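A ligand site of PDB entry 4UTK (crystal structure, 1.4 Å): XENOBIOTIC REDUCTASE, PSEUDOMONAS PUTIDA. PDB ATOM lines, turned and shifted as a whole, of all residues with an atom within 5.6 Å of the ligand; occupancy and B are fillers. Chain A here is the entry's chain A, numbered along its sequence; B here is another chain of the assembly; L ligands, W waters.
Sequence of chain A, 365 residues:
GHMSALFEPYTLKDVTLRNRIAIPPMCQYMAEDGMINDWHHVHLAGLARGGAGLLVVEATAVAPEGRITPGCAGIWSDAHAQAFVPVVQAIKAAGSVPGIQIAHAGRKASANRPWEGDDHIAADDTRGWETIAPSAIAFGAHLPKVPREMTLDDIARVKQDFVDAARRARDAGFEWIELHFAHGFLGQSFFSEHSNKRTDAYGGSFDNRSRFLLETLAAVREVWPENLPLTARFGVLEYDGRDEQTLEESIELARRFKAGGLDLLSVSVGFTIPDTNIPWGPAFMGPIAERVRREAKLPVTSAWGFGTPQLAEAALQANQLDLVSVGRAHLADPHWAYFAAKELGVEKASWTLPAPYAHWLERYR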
ATOM      1  N   PRO A  24      10.281 -25.480   3.530  1.00  0.00           N
ATOM      2  CA  PRO A  24      10.215 -24.032   3.727  1.00  0.00           C
ATOM      3  C   PRO A  24      11.078 -23.340   2.702  1.00  0.00           C
ATOM      4  O   PRO A  24      11.929 -23.979   2.088  1.00  0.00           O
ATOM      5  CB  PRO A  24      10.812 -23.835   5.129  1.00  0.00           C
ATOM      6  CG  PRO A  24      11.769 -24.976   5.270  1.00  0.00           C
ATOM      7  CD  PRO A  24      11.128 -26.140   4.547  1.00  0.00           C
ATOM      8  N   PRO A  25      10.884 -22.022   2.534  1.00  0.00           N
ATOM      9  CA  PRO A  25      11.712 -21.266   1.606  1.00  0.00           C
ATOM     10  C   PRO A  25      13.179 -21.353   1.998  1.00  0.00           C
ATOM     11  O   PRO A  25      13.539 -21.136   3.156  1.00  0.00           O
ATOM     12  CB  PRO A  25      11.178 -19.823   1.725  1.00  0.00           C
ATOM     13  CG  PRO A  25      10.474 -19.802   3.086  1.00  0.00           C
ATOM     14  CD  PRO A  25       9.932 -21.161   3.274  1.00  0.00           C
ATOM     15  N   MET A  26      14.026 -21.666   1.012  1.00  0.00           N
ATOM     16  CA  MET A  26      15.460 -21.749   1.223  1.00  0.00           C
ATOM     17  C   MET A  26      16.220 -21.113   0.067  1.00  0.00           C
ATOM     18  O   MET A  26      16.329 -21.695  -1.003  1.00  0.00           O
ATOM     19  CB  MET A  26      15.910 -23.218   1.407  1.00  0.00           C
ATOM     20  CG  MET A  26      15.501 -23.824   2.766  1.00  0.00           C
ATOM     21  SD  MET A  26      16.084 -25.516   2.960  1.00  0.00           S
ATOM     22  CE  MET A  26      14.966 -26.369   1.795  1.00  0.00           C
ATOM     23  N   CYS A  27      16.743 -19.921   0.307  1.00  0.00           N
ATOM     24  CA  CYS A  27      17.572 -19.232  -0.676  1.00  0.00           C
ATOM     25  C   CYS A  27      18.668 -20.110  -1.267  1.00  0.00           C
ATOM     26  O   CYS A  27      19.338 -20.862  -0.543  1.00  0.00           O
ATOM     27  CB  CYS A  27      18.221 -18.026  -0.013  1.00  0.00           C
ATOM     28  SG  CYS A  27      17.077 -16.624   0.135  1.00  0.00           S
ATOM     29  N   GLN A  28      18.823 -20.037  -2.588  1.00  0.00           N
ATOM     30  CA  GLN A  28      19.838 -20.786  -3.308  1.00  0.00           C
ATOM     31  C   GLN A  28      21.019 -19.923  -3.771  1.00  0.00           C
ATOM     32  O   GLN A  28      22.097 -20.453  -4.093  1.00  0.00           O
ATOM     33  CB  GLN A  28      19.184 -21.508  -4.508  1.00  0.00           C
ATOM     34  CG  GLN A  28      18.149 -22.523  -4.102  1.00  0.00           C
ATOM     35  CD  GLN A  28      18.740 -23.650  -3.341  1.00  0.00           C
ATOM     36  OE1 GLN A  28      19.399 -24.508  -3.905  1.00  0.00           O
ATOM     37  NE2 GLN A  28      18.529 -23.653  -2.012  1.00  0.00           N
ATOM     38  N   TYR A  29      20.812 -18.623  -3.838  1.00  0.00           N
ATOM     39  CA  TYR A  29      21.876 -17.674  -4.209  1.00  0.00           C
ATOM     40  C   TYR A  29      22.425 -17.932  -5.609  1.00  0.00           C
ATOM     41  O   TYR A  29      23.587 -17.628  -5.863  1.00  0.00           O
ATOM     42  CB  TYR A  29      22.996 -17.685  -3.150  1.00  0.00           C
ATOM     43  CG  TYR A  29      22.477 -17.519  -1.742  1.00  0.00           C
ATOM     44  CD1 TYR A  29      22.256 -16.269  -1.202  1.00  0.00           C
ATOM     45  CD2 TYR A  29      22.190 -18.626  -0.950  1.00  0.00           C
ATOM     46  CE1 TYR A  29      21.770 -16.139   0.092  1.00  0.00           C
ATOM     47  CE2 TYR A  29      21.721 -18.497   0.328  1.00  0.00           C
ATOM     48  CZ  TYR A  29      21.511 -17.254   0.849  1.00  0.00           C
ATOM     49  OH  TYR A  29      21.022 -17.136   2.136  1.00  0.00           O
ATOM     50  N   GLU A  58      12.053 -20.109  -2.309  1.00  0.00           N
ATOM     51  CA  GLU A  58      12.901 -19.228  -1.534  1.00  0.00           C
ATOM     52  C   GLU A  58      12.479 -17.748  -1.560  1.00  0.00           C
ATOM     53  O   GLU A  58      11.772 -17.339  -2.465  1.00  0.00           O
ATOM     54  CB  GLU A  58      14.306 -19.280  -2.112  1.00  0.00           C
ATOM     55  CG  GLU A  58      14.410 -18.783  -3.566  1.00  0.00           C
ATOM     56  CD  GLU A  58      15.718 -19.216  -4.216  1.00  0.00           C
ATOM     57  OE1 GLU A  58      16.743 -18.510  -4.057  1.00  0.00           O
ATOM     58  OE2 GLU A  58      15.730 -20.284  -4.847  1.00  0.00           O
ATOM     59  N   ALA A  59      12.914 -16.979  -0.557  1.00  0.00           N
ATOM     60  CA  ALA A  59      12.693 -15.544  -0.526  1.00  0.00           C
ATOM     61  C   ALA A  59      12.951 -14.911  -1.881  1.00  0.00           C
ATOM     62  O   ALA A  59      14.087 -14.896  -2.369  1.00  0.00           O
ATOM     63  CB  ALA A  59      13.600 -14.886   0.542  1.00  0.00           C
ATOM     64  N   GLN A 101       7.613 -17.433  -1.304  1.00  0.00           N
ATOM     65  CA  GLN A 101       7.799 -16.416  -0.283  1.00  0.00           C
ATOM     66  C   GLN A 101       8.283 -15.142  -0.943  1.00  0.00           C
ATOM     67  O   GLN A 101       9.305 -15.152  -1.613  1.00  0.00           O
ATOM     68  CB  GLN A 101       8.809 -16.886   0.779  1.00  0.00           C
ATOM     69  CG  GLN A 101       8.963 -15.914   1.913  1.00  0.00           C
ATOM     70  CD  GLN A 101      10.120 -16.261   2.790  1.00  0.00           C
ATOM     71  OE1 GLN A 101      11.254 -16.285   2.326  1.00  0.00           O
ATOM     72  NE2 GLN A 101       9.840 -16.566   4.043  1.00  0.00           N
ATOM     73  N   GLU A 178       3.566 -16.599   0.780  1.00  0.00           N
ATOM     74  CA  GLU A 178       4.075 -16.298   2.111  1.00  0.00           C
ATOM     75  C   GLU A 178       4.750 -14.945   2.127  1.00  0.00           C
ATOM     76  O   GLU A 178       5.709 -14.706   1.400  1.00  0.00           O
ATOM     77  CB  GLU A 178       5.062 -17.370   2.575  1.00  0.00           C
ATOM     78  CG  GLU A 178       5.487 -17.158   4.049  1.00  0.00           C
ATOM     79  CD  GLU A 178       6.406 -18.258   4.561  1.00  0.00           C
ATOM     80  OE1 GLU A 178       5.920 -19.360   4.861  1.00  0.00           O
ATOM     81  OE2 GLU A 178       7.622 -18.007   4.705  1.00  0.00           O
ATOM     82  N   HIS A 180       7.205 -12.475   3.755  1.00  0.00           N
ATOM     83  CA  HIS A 180       8.372 -12.627   4.608  1.00  0.00           C
ATOM     84  C   HIS A 180       8.518 -11.449   5.547  1.00  0.00           C
ATOM     85  O   HIS A 180       9.231 -10.476   5.259  1.00  0.00           O
ATOM     86  CB  HIS A 180       9.644 -12.802   3.766  1.00  0.00           C
ATOM     87  CG  HIS A 180      10.793 -13.359   4.551  1.00  0.00           C
ATOM     88  ND1 HIS A 180      10.766 -13.478   5.922  1.00  0.00           N
ATOM     89  CD2 HIS A 180      11.975 -13.893   4.142  1.00  0.00           C
ATOM     90  CE1 HIS A 180      11.900 -14.038   6.324  1.00  0.00           C
ATOM     91  NE2 HIS A 180      12.638 -14.304   5.271  1.00  0.00           N
ATOM     92  N   HIS A 183      13.007 -12.676  10.255  1.00  0.00           N
ATOM     93  CA  HIS A 183      14.459 -12.761  10.100  1.00  0.00           C
ATOM     94  C   HIS A 183      15.154 -11.396   9.952  1.00  0.00           C
ATOM     95  O   HIS A 183      16.209 -11.282   9.329  1.00  0.00           O
ATOM     96  CB  HIS A 183      14.805 -13.726   8.965  1.00  0.00           C
ATOM     97  CG  HIS A 183      14.164 -15.066   9.129  1.00  0.00           C
ATOM     98  ND1 HIS A 183      14.157 -16.021   8.129  1.00  0.00           N
ATOM     99  CD2 HIS A 183      13.504 -15.615  10.185  1.00  0.00           C
ATOM    100  CE1 HIS A 183      13.527 -17.098   8.561  1.00  0.00           C
ATOM    101  NE2 HIS A 183      13.122 -16.873   9.800  1.00  0.00           N
ATOM    102  N   ARG A 233       5.479 -15.341   7.317  1.00  0.00           N
ATOM    103  CA  ARG A 233       6.481 -15.765   8.277  1.00  0.00           C
ATOM    104  C   ARG A 233       6.765 -14.578   9.155  1.00  0.00           C
ATOM    105  O   ARG A 233       6.905 -13.452   8.672  1.00  0.00           O
ATOM    106  CB  ARG A 233       7.770 -16.226   7.578  1.00  0.00           C
ATOM    107  CG  ARG A 233       8.668 -17.036   8.502  1.00  0.00           C
ATOM    108  CD  ARG A 233       9.717 -17.843   7.774  1.00  0.00           C
ATOM    109  NE  ARG A 233       9.910 -19.108   8.442  1.00  0.00           N
ATOM    110  CZ  ARG A 233      10.816 -20.011   8.107  1.00  0.00           C
ATOM    111  NH1 ARG A 233      11.662 -19.769   7.106  1.00  0.00           N
ATOM    112  NH2 ARG A 233      10.852 -21.145   8.785  1.00  0.00           N
ATOM    113  N   SER A 268       8.632 -18.052  13.562  1.00  0.00           N
ATOM    114  CA  SER A 268      10.082 -18.106  13.524  1.00  0.00           C
ATOM    115  C   SER A 268      10.649 -17.224  14.628  1.00  0.00           C
ATOM    116  O   SER A 268       9.924 -16.721  15.513  1.00  0.00           O
ATOM    117  CB  SER A 268      10.578 -17.687  12.137  1.00  0.00           C
ATOM    118  OG  SER A 268      11.901 -18.134  11.871  1.00  0.00           O
ATOM    119  N   ALA A 303       9.956 -24.451  12.112  1.00  0.00           N
ATOM    120  CA  ALA A 303      11.120 -25.133  11.568  1.00  0.00           C
ATOM    121  C   ALA A 303      12.221 -25.013  12.604  1.00  0.00           C
ATOM    122  O   ALA A 303      11.954 -24.735  13.749  1.00  0.00           O
ATOM    123  CB  ALA A 303      11.573 -24.479  10.241  1.00  0.00           C
ATOM    124  N   TRP A 304      13.464 -25.172  12.176  1.00  0.00           N
ATOM    125  CA  TRP A 304      14.643 -24.981  13.046  1.00  0.00           C
ATOM    126  C   TRP A 304      14.813 -26.146  13.998  1.00  0.00           C
ATOM    127  O   TRP A 304      15.025 -25.938  15.207  1.00  0.00           O
ATOM    128  CB  TRP A 304      14.608 -23.649  13.823  1.00  0.00           C
ATOM    129  CG  TRP A 304      14.369 -22.402  12.986  1.00  0.00           C
ATOM    130  CD1 TRP A 304      13.206 -21.693  12.899  1.00  0.00           C
ATOM    131  CD2 TRP A 304      15.320 -21.735  12.154  1.00  0.00           C
ATOM    132  NE1 TRP A 304      13.363 -20.633  12.048  1.00  0.00           N
ATOM    133  CE2 TRP A 304      14.648 -20.632  11.577  1.00  0.00           C
ATOM    134  CE3 TRP A 304      16.659 -21.967  11.826  1.00  0.00           C
ATOM    135  CZ2 TRP A 304      15.290 -19.753  10.695  1.00  0.00           C
ATOM    136  CZ3 TRP A 304      17.289 -21.093  10.955  1.00  0.00           C
ATOM    137  CH2 TRP A 304      16.599 -20.006  10.397  1.00  0.00           C
ATOM    138  N   GLY A 305      14.718 -27.359  13.469  1.00  0.00           N
ATOM    139  CA  GLY A 305      15.015 -28.545  14.247  1.00  0.00           C
ATOM    140  C   GLY A 305      13.976 -29.650  14.287  1.00  0.00           C
ATOM    141  O   GLY A 305      14.025 -30.490  15.180  1.00  0.00           O
ATOM    142  N   PHE A 306      13.047 -29.669  13.334  1.00  0.00           N
ATOM    143  CA  PHE A 306      12.025 -30.716  13.287  1.00  0.00           C
ATOM    144  C   PHE A 306      12.388 -31.789  12.261  1.00  0.00           C
ATOM    145  O   PHE A 306      11.595 -32.670  11.977  1.00  0.00           O
ATOM    146  CB  PHE A 306      10.647 -30.126  12.934  1.00  0.00           C
ATOM    147  CG  PHE A 306      10.060 -29.227  13.999  1.00  0.00           C
ATOM    148  CD1 PHE A 306       9.333 -29.754  15.047  1.00  0.00           C
ATOM    149  CD2 PHE A 306      10.205 -27.859  13.917  1.00  0.00           C
ATOM    150  CE1 PHE A 306       8.779 -28.913  16.008  1.00  0.00           C
ATOM    151  CE2 PHE A 306       9.685 -27.024  14.866  1.00  0.00           C
ATOM    152  CZ  PHE A 306       8.954 -27.541  15.898  1.00  0.00           C
ATOM    153  N   GLY A 307      13.598 -31.748  11.712  1.00  0.00           N
ATOM    154  CA  GLY A 307      13.937 -32.631  10.606  1.00  0.00           C
ATOM    155  C   GLY A 307      14.372 -34.049  10.945  1.00  0.00           C
ATOM    156  O   GLY A 307      15.355 -34.532  10.398  1.00  0.00           O
ATOM    157  N   SER A 325       7.705 -27.888   8.853  1.00  0.00           N
ATOM    158  CA  SER A 325       8.659 -27.418   7.850  1.00  0.00           C
ATOM    159  C   SER A 325      10.003 -28.099   8.057  1.00  0.00           C
ATOM    160  O   SER A 325      10.543 -28.075   9.149  1.00  0.00           O
ATOM    161  CB  SER A 325       8.806 -25.914   7.901  1.00  0.00           C
ATOM    162  OG  SER A 325       7.566 -25.317   7.545  1.00  0.00           O
ATOM    163  N   VAL A 326      10.526 -28.716   6.991  1.00  0.00           N
ATOM    164  CA  VAL A 326      11.775 -29.472   7.041  1.00  0.00           C
ATOM    165  C   VAL A 326      12.685 -28.964   5.939  1.00  0.00           C
ATOM    166  O   VAL A 326      12.442 -29.206   4.753  1.00  0.00           O
ATOM    167  CB  VAL A 326      11.507 -30.971   6.841  1.00  0.00           C
ATOM    168  CG1 VAL A 326      12.820 -31.782   6.854  1.00  0.00           C
ATOM    169  CG2 VAL A 326      10.563 -31.481   7.925  1.00  0.00           C
ATOM    170  N   GLY A 327      13.752 -28.275   6.342  1.00  0.00           N
ATOM    171  CA  GLY A 327      14.587 -27.529   5.417  1.00  0.00           C
ATOM    172  C   GLY A 327      15.870 -28.249   5.074  1.00  0.00           C
ATOM    173  O   GLY A 327      15.969 -28.876   4.026  1.00  0.00           O
ATOM    174  N   ARG A 328      16.878 -28.131   5.927  1.00  0.00           N
ATOM    175  CA  ARG A 328      18.178 -28.747   5.657  1.00  0.00           C
ATOM    176  C   ARG A 328      18.148 -30.238   5.359  1.00  0.00           C
ATOM    177  O   ARG A 328      18.932 -30.690   4.541  1.00  0.00           O
ATOM    178  CB  ARG A 328      19.154 -28.431   6.783  1.00  0.00           C
ATOM    179  CG  ARG A 328      19.610 -26.971   6.725  1.00  0.00           C
ATOM    180  CD  ARG A 328      20.327 -26.553   7.949  1.00  0.00           C
ATOM    181  NE  ARG A 328      19.426 -26.520   9.085  1.00  0.00           N
ATOM    182  CZ  ARG A 328      19.789 -26.233  10.321  1.00  0.00           C
ATOM    183  NH1 ARG A 328      21.049 -25.979  10.589  1.00  0.00           N
ATOM    184  NH2 ARG A 328      18.878 -26.230  11.285  1.00  0.00           N
ATOM    185  N   ALA A 329      17.250 -30.999   5.977  1.00  0.00           N
ATOM    186  CA  ALA A 329      17.204 -32.433   5.671  1.00  0.00           C
ATOM    187  C   ALA A 329      16.874 -32.701   4.200  1.00  0.00           C
ATOM    188  O   ALA A 329      17.247 -33.730   3.655  1.00  0.00           O
ATOM    189  CB  ALA A 329      16.243 -33.146   6.585  1.00  0.00           C
ATOM    190  N   LEU A 331      17.887 -30.655   1.717  1.00  0.00           N
ATOM    191  CA  LEU A 331      19.112 -30.373   0.979  1.00  0.00           C
ATOM    192  C   LEU A 331      20.011 -31.616   0.997  1.00  0.00           C
ATOM    193  O   LEU A 331      20.610 -31.980  -0.025  1.00  0.00           O
ATOM    194  CB  LEU A 331      19.843 -29.151   1.526  1.00  0.00           C
ATOM    195  CG  LEU A 331      19.020 -27.865   1.684  1.00  0.00           C
ATOM    196  CD1 LEU A 331      19.888 -26.752   2.228  1.00  0.00           C
ATOM    197  CD2 LEU A 331      18.405 -27.450   0.355  1.00  0.00           C
ATOM    198  N   PRO B 356      25.290 -24.413  -2.855  1.00  0.00           N
ATOM    199  CA  PRO B 356      24.019 -24.016  -2.236  1.00  0.00           C
ATOM    200  C   PRO B 356      23.448 -25.075  -1.290  1.00  0.00           C
ATOM    201  O   PRO B 356      22.505 -24.797  -0.531  1.00  0.00           O
ATOM    202  CB  PRO B 356      23.077 -23.787  -3.439  1.00  0.00           C
ATOM    203  CG  PRO B 356      24.002 -23.561  -4.599  1.00  0.00           C
ATOM    204  CD  PRO B 356      25.221 -24.401  -4.331  1.00  0.00           C
ATOM    205  N   TRP B 360      25.530 -25.390   3.979  1.00  0.00           N
ATOM    206  CA  TRP B 360      24.585 -25.523   5.082  1.00  0.00           C
ATOM    207  C   TRP B 360      24.683 -26.837   5.814  1.00  0.00           C
ATOM    208  O   TRP B 360      24.167 -26.975   6.924  1.00  0.00           O
ATOM    209  CB  TRP B 360      23.174 -25.371   4.525  1.00  0.00           C
ATOM    210  CG  TRP B 360      23.036 -24.116   3.778  1.00  0.00           C
ATOM    211  CD1 TRP B 360      22.961 -23.955   2.432  1.00  0.00           C
ATOM    212  CD2 TRP B 360      23.038 -22.810   4.338  1.00  0.00           C
ATOM    213  NE1 TRP B 360      22.893 -22.618   2.116  1.00  0.00           N
ATOM    214  CE2 TRP B 360      22.936 -21.895   3.276  1.00  0.00           C
ATOM    215  CE3 TRP B 360      23.113 -22.325   5.642  1.00  0.00           C
ATOM    216  CZ2 TRP B 360      22.894 -20.532   3.485  1.00  0.00           C
ATOM    217  CZ3 TRP B 360      23.083 -20.975   5.841  1.00  0.00           C
ATOM    218  CH2 TRP B 360      22.980 -20.089   4.773  1.00  0.00           C
HETATM  219  C1  LIG L   1      16.963 -20.846   4.803  1.00  0.00           C
HETATM  220  N1  LIG L   1      15.937 -20.163   5.568  1.00  0.00           N
HETATM  221  C2  LIG L   1      15.197 -19.277   4.955  1.00  0.00           C
HETATM  222  N2  LIG L   1      14.085 -18.823   5.539  1.00  0.00           N
HETATM  223  C3  LIG L   1      13.272 -18.015   4.894  1.00  0.00           C
HETATM  224  O1  LIG L   1      12.242 -17.597   5.520  1.00  0.00           O
HETATM  225  N3  LIG L   1      13.465 -17.692   3.672  1.00  0.00           N
HETATM  226  C4  LIG L   1      14.531 -18.149   2.978  1.00  0.00           C
HETATM  227  O2  LIG L   1      14.615 -17.895   1.786  1.00  0.00           O
HETATM  228  C5  LIG L   1      15.529 -18.784   3.736  1.00  0.00           C
HETATM  229  N4  LIG L   1      16.768 -19.111   3.228  1.00  0.00           N
HETATM  230  C6  LIG L   1      17.319 -20.317   3.684  1.00  0.00           C
HETATM  231  C7  LIG L   1      18.312 -20.904   2.961  1.00  0.00           C
HETATM  232  C8  LIG L   1      18.731 -22.132   3.290  1.00  0.00           C
HETATM  233  C9  LIG L   1      19.788 -22.766   2.464  1.00  0.00           C
HETATM  234  C10 LIG L   1      18.526 -22.497   4.488  1.00  0.00           C
HETATM  235  C11 LIG L   1      19.090 -23.843   5.010  1.00  0.00           C
HETATM  236  C12 LIG L   1      17.596 -21.867   5.235  1.00  0.00           C
HETATM  237  C13 LIG L   1      15.438 -20.862   6.854  1.00  0.00           C
HETATM  238  C14 LIG L   1      14.694 -22.143   6.537  1.00  0.00           C
HETATM  239  O3  LIG L   1      13.459 -21.892   5.953  1.00  0.00           O
HETATM  240  C15 LIG L   1      14.416 -22.956   7.809  1.00  0.00           C
HETATM  241  O4  LIG L   1      13.726 -22.130   8.743  1.00  0.00           O
HETATM  242  C16 LIG L   1      15.670 -23.490   8.476  1.00  0.00           C
HETATM  243  O5  LIG L   1      16.360 -24.210   7.476  1.00  0.00           O
HETATM  244  C17 LIG L   1      15.384 -24.346   9.712  1.00  0.00           C
HETATM  245  O6  LIG L   1      14.715 -25.535   9.375  1.00  0.00           O
HETATM  246  P1  LIG L   1      15.585 -26.917   9.326  1.00  0.00           P
HETATM  247  O7  LIG L   1      16.685 -26.680   8.360  1.00  0.00           O
HETATM  248  O8  LIG L   1      16.140 -27.144  10.617  1.00  0.00           O
HETATM  249  O9  LIG L   1      14.646 -27.918   8.916  1.00  0.00           O
HETATM  250  O   HOH W   1      15.640 -29.875  11.479  1.00  0.00           O
HETATM  251  O   HOH W   2      15.296 -15.812   5.590  1.00  0.00           O
HETATM  252  O   HOH W   3      17.989 -29.296  11.055  1.00  0.00           O
HETATM  253  O   HOH W   4      12.716 -28.262  10.819  1.00  0.00           O
HETATM  254  O   HOH W   5      15.926 -30.395   8.428  1.00  0.00           O
HETATM  255  O   HOH W   6      18.552 -16.540   3.092  1.00  0.00           O
HETATM  256  O   HOH W   7      19.316 -20.382   7.820  1.00  0.00           O
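NH1 of Arg 233 is in hydrogen-bond range of O1 of the ligand, 2.8 Å away. An oxygen (O2) of the ligand sits close to the backbone NH (N) of Cys 27, at 3.3 Å. NE of Arg 328 is in salt-bridge range of O7 of the ligand. O8 of the ligand lies within hydrogen-bond range of N of Gly 305, at 3.2 Å. SG of Cys 27 is in hydrogen-bond range of O2 of the ligand, 3.2 Å away. OE1 of Gln 101 sits at hydrogen-bond distance from N3 of the ligand. The backbone NH (N) of Trp 304 is in hydrogen-bond range of an oxygen (O6) of the ligand. N of Arg 328 lies within hydrogen-bond range of O7 of the ligand (2.8 Å). The backbone NH of Ala 59 lies within hydrogen-bond range of an oxygen (O2) of the ligand (3.0 Å). NE2 of His 180 sits at hydrogen-bond distance from O1 of the ligand (3.3 Å). An oxygen (O3) of the ligand sits at hydrogen-bond distance from the backbone carbonyl oxygen (O) of Pro 25, 2.9 Å away. An oxygen (O9) of the ligand is in hydrogen-bond range of the backbone NH (N) of Gly 327 (2.7 Å).
NE2 of His 183 lies within hydrogen-bond range of OG of Ser 268 (2.7 Å). The side-chain amide oxygen (OE1) of Gln 101 sits close to the backbone NH (N) of Ala 59. The backbone carbonyl oxygen of Pro 356 of chain B lies close to the indole nitrogen of Trp 360 of chain B, at 3.5 Å. OE1 of Glu 58 sits at hydrogen-bond distance from N of Gln 28, at 3.0 Å. OG of Ser 268 is in hydrogen-bond range of NE1 of Trp 304 (2.9 Å). The side-chain amide nitrogen of Gln 28 sits at hydrogen-bond distance from the backbone carbonyl oxygen of Met 26 (3.1 Å). The side-chain amide nitrogen (NE2) of Gln 101 sits at hydrogen-bond distance from the side-chain carboxylate (OE2) of Glu 178, at 2.7 Å.
Residues that only touch the ligand: Pro 24 (3.4 Å), Met 26 (3.4 Å), Glu 58 (3.97 Å), His 183 (3.3 Å), Ala 303 (3.4 Å), Val 326 (3.7 Å), Leu 331 (3.99 Å) and Trp 360 of chain B (3.1 Å). 18 residues have an atom within 4 Å of the ligand: Pro 24, Pro 25, Met 26, Cys 27, Glu 58, Ala 59, Gln 101, His 180, His 183, Arg 233, Ala 303, Trp 304, Gly 305, Val 326, Gly 327, Arg 328, Leu 331 and Trp 360 of chain B. The nearest printed residue that does not touch the ligand is Ser 325 (4.1 Å).
Water W5 bridges an oxygen (O9) of the ligand (2.8 Å) and the backbone NH (N) of Ala 329 (2.9 Å). Water W3 lies within hydrogen-bond range of O8 of the ligand (2.9 Å) and NH2 of Arg 328 (3.2 Å). Water W2 lies within hydrogen-bond range of ND1 of His 183 (2.8 Å), NE2 of His 180 (3.1 Å) and N2 of the ligand (3.2 Å). Water W6 lies within hydrogen-bond range of OH of Tyr 29 (2.7 Å), N4 of the ligand (3.1 Å) and SG of Cys 27 (3.3 Å).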
